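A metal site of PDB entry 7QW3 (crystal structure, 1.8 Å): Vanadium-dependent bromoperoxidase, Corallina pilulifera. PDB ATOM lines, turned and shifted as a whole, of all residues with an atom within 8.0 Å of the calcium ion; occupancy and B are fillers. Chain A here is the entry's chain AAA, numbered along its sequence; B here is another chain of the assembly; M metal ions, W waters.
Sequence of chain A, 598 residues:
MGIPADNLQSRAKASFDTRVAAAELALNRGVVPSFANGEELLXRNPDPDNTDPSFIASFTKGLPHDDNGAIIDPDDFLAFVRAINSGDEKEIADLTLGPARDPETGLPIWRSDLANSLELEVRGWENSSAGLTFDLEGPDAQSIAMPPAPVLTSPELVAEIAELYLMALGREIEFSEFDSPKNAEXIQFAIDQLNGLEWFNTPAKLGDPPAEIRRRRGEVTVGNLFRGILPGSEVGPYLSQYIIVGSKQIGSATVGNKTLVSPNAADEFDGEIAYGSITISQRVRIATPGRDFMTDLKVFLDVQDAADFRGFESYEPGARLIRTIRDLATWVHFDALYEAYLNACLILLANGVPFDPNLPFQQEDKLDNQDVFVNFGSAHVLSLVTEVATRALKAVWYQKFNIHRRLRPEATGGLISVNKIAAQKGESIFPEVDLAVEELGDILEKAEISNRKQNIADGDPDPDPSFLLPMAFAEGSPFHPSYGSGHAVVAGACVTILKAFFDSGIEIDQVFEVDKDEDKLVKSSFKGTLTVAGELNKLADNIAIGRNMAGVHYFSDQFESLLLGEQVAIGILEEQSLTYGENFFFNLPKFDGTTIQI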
ATOM      1  N   PRO A 360      27.685   5.441  24.386  1.00  0.00           N
ATOM      2  CA  PRO A 360      26.371   4.938  23.982  1.00  0.00           C
ATOM      3  C   PRO A 360      25.860   3.924  24.988  1.00  0.00           C
ATOM      4  O   PRO A 360      26.641   3.329  25.759  1.00  0.00           O
ATOM      5  CB  PRO A 360      26.622   4.202  22.645  1.00  0.00           C
ATOM      6  CG  PRO A 360      28.069   4.536  22.264  1.00  0.00           C
ATOM      7  CD  PRO A 360      28.775   4.837  23.583  1.00  0.00           C
ATOM      8  N   PHE A 361      24.519   3.754  24.985  1.00  0.00           N
ATOM      9  CA  PHE A 361      23.854   2.583  25.588  1.00  0.00           C
ATOM     10  C   PHE A 361      23.890   2.603  27.127  1.00  0.00           C
ATOM     11  O   PHE A 361      23.624   1.574  27.748  1.00  0.00           O
ATOM     12  CB  PHE A 361      24.441   1.265  25.064  1.00  0.00           C
ATOM     13  CG  PHE A 361      24.483   1.162  23.554  1.00  0.00           C
ATOM     14  CD1 PHE A 361      23.380   1.525  22.773  1.00  0.00           C
ATOM     15  CD2 PHE A 361      25.594   0.623  22.917  1.00  0.00           C
ATOM     16  CE1 PHE A 361      23.415   1.391  21.374  1.00  0.00           C
ATOM     17  CE2 PHE A 361      25.622   0.496  21.535  1.00  0.00           C
ATOM     18  CZ  PHE A 361      24.536   0.858  20.763  1.00  0.00           C
ATOM     19  N   GLN A 362      24.128   3.788  27.694  1.00  0.00           N
ATOM     20  CA  GLN A 362      24.267   3.910  29.145  1.00  0.00           C
ATOM     21  C   GLN A 362      22.915   4.102  29.837  1.00  0.00           C
ATOM     22  O   GLN A 362      22.864   4.189  31.064  1.00  0.00           O
ATOM     23  CB  GLN A 362      25.289   4.979  29.527  1.00  0.00           C
ATOM     24  CG  GLN A 362      26.661   4.727  28.901  1.00  0.00           C
ATOM     25  CD  GLN A 362      27.346   3.416  29.249  1.00  0.00           C
ATOM     26  OE1 GLN A 362      27.225   2.902  30.365  1.00  0.00           O
ATOM     27  NE2 GLN A 362      28.119   2.911  28.291  1.00  0.00           N
ATOM     28  N   GLN A 363      21.834   4.178  29.070  1.00  0.00           N
ATOM     29  CA  GLN A 363      20.526   4.371  29.688  1.00  0.00           C
ATOM     30  C   GLN A 363      19.994   3.014  30.151  1.00  0.00           C
ATOM     31  O   GLN A 363      20.528   1.947  29.797  1.00  0.00           O
ATOM     32  CB  GLN A 363      19.550   4.910  28.653  1.00  0.00           C
ATOM     33  CG  GLN A 363      19.896   6.347  28.255  1.00  0.00           C
ATOM     34  CD  GLN A 363      19.014   6.770  27.108  1.00  0.00           C
ATOM     35  OE1 GLN A 363      19.335   6.511  25.930  1.00  0.00           O
ATOM     36  NE2 GLN A 363      17.884   7.366  27.452  1.00  0.00           N
ATOM     37  N   GLU A 364      18.895   3.073  30.939  1.00  0.00           N
ATOM     38  CA  GLU A 364      18.182   1.859  31.320  1.00  0.00           C
ATOM     39  C   GLU A 364      17.786   1.113  30.055  1.00  0.00           C
ATOM     40  O   GLU A 364      17.385   1.735  29.075  1.00  0.00           O
ATOM     41  CB  GLU A 364      16.918   2.223  32.120  1.00  0.00           C
ATOM     42  CG  GLU A 364      17.265   2.886  33.430  1.00  0.00           C
ATOM     43  CD  GLU A 364      16.157   2.953  34.463  1.00  0.00           C
ATOM     44  OE1 GLU A 364      16.443   3.496  35.565  1.00  0.00           O
ATOM     45  OE2 GLU A 364      15.034   2.464  34.177  1.00  0.00           O
ATOM     46  N   ASP A 365      17.892  -0.216  30.094  1.00  0.00           N
ATOM     47  CA  ASP A 365      17.727  -1.000  28.869  1.00  0.00           C
ATOM     48  C   ASP A 365      16.304  -0.912  28.335  1.00  0.00           C
ATOM     49  O   ASP A 365      16.082  -1.114  27.132  1.00  0.00           O
ATOM     50  CB  ASP A 365      18.187  -2.426  29.134  1.00  0.00           C
ATOM     51  CG  ASP A 365      19.718  -2.490  29.279  1.00  0.00           C
ATOM     52  OD1 ASP A 365      20.409  -1.420  29.045  1.00  0.00           O
ATOM     53  OD2 ASP A 365      20.203  -3.581  29.578  1.00  0.00           O
ATOM     54  N   LYS A 366      15.326  -0.591  29.199  1.00  0.00           N
ATOM     55  CA  LYS A 366      13.966  -0.447  28.682  1.00  0.00           C
ATOM     56  C   LYS A 366      13.896   0.714  27.681  1.00  0.00           C
ATOM     57  O   LYS A 366      13.002   0.735  26.828  1.00  0.00           O
ATOM     58  CB  LYS A 366      12.939  -0.242  29.810  1.00  0.00           C
ATOM     59  CG  LYS A 366      13.056   1.069  30.577  1.00  0.00           C
ATOM     60  CD  LYS A 366      11.812   1.324  31.460  1.00  0.00           C
ATOM     61  CE  LYS A 366      11.919   2.607  32.269  1.00  0.00           C
ATOM     62  NZ  LYS A 366      10.652   2.906  32.989  1.00  0.00           N
ATOM     63  N   LEU A 367      14.866   1.654  27.758  1.00  0.00           N
ATOM     64  CA  LEU A 367      14.869   2.779  26.834  1.00  0.00           C
ATOM     65  C   LEU A 367      15.728   2.495  25.599  1.00  0.00           C
ATOM     66  O   LEU A 367      15.296   2.796  24.475  1.00  0.00           O
ATOM     67  CB  LEU A 367      15.366   4.036  27.548  1.00  0.00           C
ATOM     68  CG  LEU A 367      14.521   4.469  28.756  1.00  0.00           C
ATOM     69  CD1 LEU A 367      15.135   5.724  29.404  1.00  0.00           C
ATOM     70  CD2 LEU A 367      13.086   4.722  28.305  1.00  0.00           C
ATOM     71  N   ASP A 368      16.907   1.880  25.785  1.00  0.00           N
ATOM     72  CA  ASP A 368      17.853   1.780  24.665  1.00  0.00           C
ATOM     73  C   ASP A 368      17.975   0.360  24.104  1.00  0.00           C
ATOM     74  O   ASP A 368      18.639   0.156  23.079  1.00  0.00           O
ATOM     75  CB  ASP A 368      19.228   2.354  25.067  1.00  0.00           C
ATOM     76  CG  ASP A 368      19.958   1.696  26.241  1.00  0.00           C
ATOM     77  OD1 ASP A 368      19.618   0.572  26.661  1.00  0.00           O
ATOM     78  OD2 ASP A 368      20.961   2.272  26.742  1.00  0.00           O
ATOM     79  N   ASN A 369      17.350  -0.638  24.749  1.00  0.00           N
ATOM     80  CA  ASN A 369      17.459  -2.044  24.372  1.00  0.00           C
ATOM     81  C   ASN A 369      18.926  -2.520  24.257  1.00  0.00           C
ATOM     82  O   ASN A 369      19.203  -3.392  23.428  1.00  0.00           O
ATOM     83  CB  ASN A 369      16.809  -2.356  23.023  1.00  0.00           C
ATOM     84  CG  ASN A 369      15.297  -2.170  23.057  1.00  0.00           C
ATOM     85  OD1 ASN A 369      14.701  -2.201  24.129  1.00  0.00           O
ATOM     86  ND2 ASN A 369      14.674  -1.942  21.906  1.00  0.00           N
ATOM     87  N   GLN A 370      19.846  -1.965  25.065  1.00  0.00           N
ATOM     88  CA  GLN A 370      21.220  -2.367  24.804  1.00  0.00           C
ATOM     89  C   GLN A 370      22.075  -2.191  26.058  1.00  0.00           C
ATOM     90  O   GLN A 370      22.147  -1.090  26.613  1.00  0.00           O
ATOM     91  CB  GLN A 370      21.792  -1.477  23.709  1.00  0.00           C
ATOM     92  CG  GLN A 370      23.147  -1.961  23.151  1.00  0.00           C
ATOM     93  CD  GLN A 370      23.107  -3.076  22.124  1.00  0.00           C
ATOM     94  OE1 GLN A 370      24.148  -3.420  21.558  1.00  0.00           O
ATOM     95  NE2 GLN A 370      21.938  -3.640  21.802  1.00  0.00           N
ATOM     96  N   ASP A 371      22.722  -3.287  26.460  1.00  0.00           N
ATOM     97  CA  ASP A 371      23.660  -3.254  27.573  1.00  0.00           C
ATOM     98  C   ASP A 371      25.076  -3.253  26.972  1.00  0.00           C
ATOM     99  O   ASP A 371      25.227  -3.368  25.762  1.00  0.00           O
ATOM    100  CB  ASP A 371      23.408  -4.479  28.444  1.00  0.00           C
ATOM    101  CG  ASP A 371      24.034  -4.468  29.838  1.00  0.00           C
ATOM    102  OD1 ASP A 371      24.702  -3.485  30.211  1.00  0.00           O
ATOM    103  OD2 ASP A 371      23.856  -5.487  30.560  1.00  0.00           O
ATOM    104  N   VAL A 372      26.075  -3.051  27.830  1.00  0.00           N
ATOM    105  CA  VAL A 372      27.430  -2.825  27.338  1.00  0.00           C
ATOM    106  C   VAL A 372      28.396  -3.840  27.929  1.00  0.00           C
ATOM    107  O   VAL A 372      28.215  -4.258  29.076  1.00  0.00           O
ATOM    108  CB  VAL A 372      27.891  -1.389  27.650  1.00  0.00           C
ATOM    109  CG1 VAL A 372      27.127  -0.394  26.771  1.00  0.00           C
ATOM    110  CG2 VAL A 372      27.740  -1.026  29.133  1.00  0.00           C
ATOM    111  N   ARG B 123      16.384  -6.567  30.604  1.00  0.00           N
ATOM    112  CA  ARG B 123      17.797  -6.292  30.288  1.00  0.00           C
ATOM    113  C   ARG B 123      17.939  -6.384  28.780  1.00  0.00           C
ATOM    114  O   ARG B 123      17.154  -7.096  28.155  1.00  0.00           O
ATOM    115  CB  ARG B 123      18.708  -7.320  30.977  1.00  0.00           C
ATOM    116  CG  ARG B 123      18.377  -8.758  30.570  1.00  0.00           C
ATOM    117  CD  ARG B 123      19.363  -9.732  31.246  1.00  0.00           C
ATOM    118  NE  ARG B 123      20.738  -9.478  30.865  1.00  0.00           N
ATOM    119  CZ  ARG B 123      21.756 -10.305  31.076  1.00  0.00           C
ATOM    120  NH1 ARG B 123      21.526 -11.507  31.605  1.00  0.00           N
ATOM    121  NH2 ARG B 123      22.998  -9.934  30.746  1.00  0.00           N
ATOM    122  N   GLY B 124      18.959  -5.702  28.220  1.00  0.00           N
ATOM    123  CA  GLY B 124      19.048  -5.585  26.772  1.00  0.00           C
ATOM    124  C   GLY B 124      20.249  -6.345  26.209  1.00  0.00           C
ATOM    125  O   GLY B 124      21.125  -6.804  26.967  1.00  0.00           O
ATOM    126  N   TRP B 125      20.298  -6.449  24.885  1.00  0.00           N
ATOM    127  CA  TRP B 125      21.410  -7.162  24.234  1.00  0.00           C
ATOM    128  C   TRP B 125      22.749  -6.465  24.519  1.00  0.00           C
ATOM    129  O   TRP B 125      22.840  -5.233  24.585  1.00  0.00           O
ATOM    130  CB  TRP B 125      21.127  -7.310  22.733  1.00  0.00           C
ATOM    131  CG  TRP B 125      19.850  -8.089  22.539  1.00  0.00           C
ATOM    132  CD1 TRP B 125      19.699  -9.442  22.711  1.00  0.00           C
ATOM    133  CD2 TRP B 125      18.551  -7.577  22.206  1.00  0.00           C
ATOM    134  NE1 TRP B 125      18.394  -9.806  22.464  1.00  0.00           N
ATOM    135  CE2 TRP B 125      17.667  -8.693  22.172  1.00  0.00           C
ATOM    136  CE3 TRP B 125      18.026  -6.299  21.935  1.00  0.00           C
ATOM    137  CZ2 TRP B 125      16.301  -8.566  21.888  1.00  0.00           C
ATOM    138  CZ3 TRP B 125      16.681  -6.168  21.680  1.00  0.00           C
ATOM    139  CH2 TRP B 125      15.822  -7.292  21.637  1.00  0.00           C
HETATM  140 CA    CA M   1      21.531   0.468  28.246  1.00  0.00          CA
HETATM  141  O   HOH W   1      22.988  -0.329  29.928  1.00  0.00           O
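The side-chain amide oxygen (OD1) of Asn 369 sits close to the backbone carbonyl oxygen (O) of Asp 365 (3.5 Å).
The backbone carbonyl oxygen (O) of Trp 125 of chain B lies close to the side-chain amide nitrogen (NE2) of Gln 370 (3.3 Å).
OD2 of Asp 365 is in hydrogen-bond range of N of Gly 124 of chain B, at 2.8 Å.
Five residues have an atom within 4 Å of the calcium ion: Phe 361, Gln 363, Asp 365, Asp 368 and Gln 370.
The calcium ion is bound by the side-chain carboxylate (OD1) of Asp 365 (2.3 Å), the backbone carbonyl oxygen (O) of Gln 370 (2.3 Å), water W1 (2.4 Å), the backbone carbonyl oxygen (O) of Gln 363 (2.4 Å), the side-chain carboxylate (OD2) of Asp 368 (2.4 Å), the backbone carbonyl oxygen (O) of Phe 361 (2.4 Å) and the side-chain carboxylate (OD1) of Asp 368 (2.5 Å).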
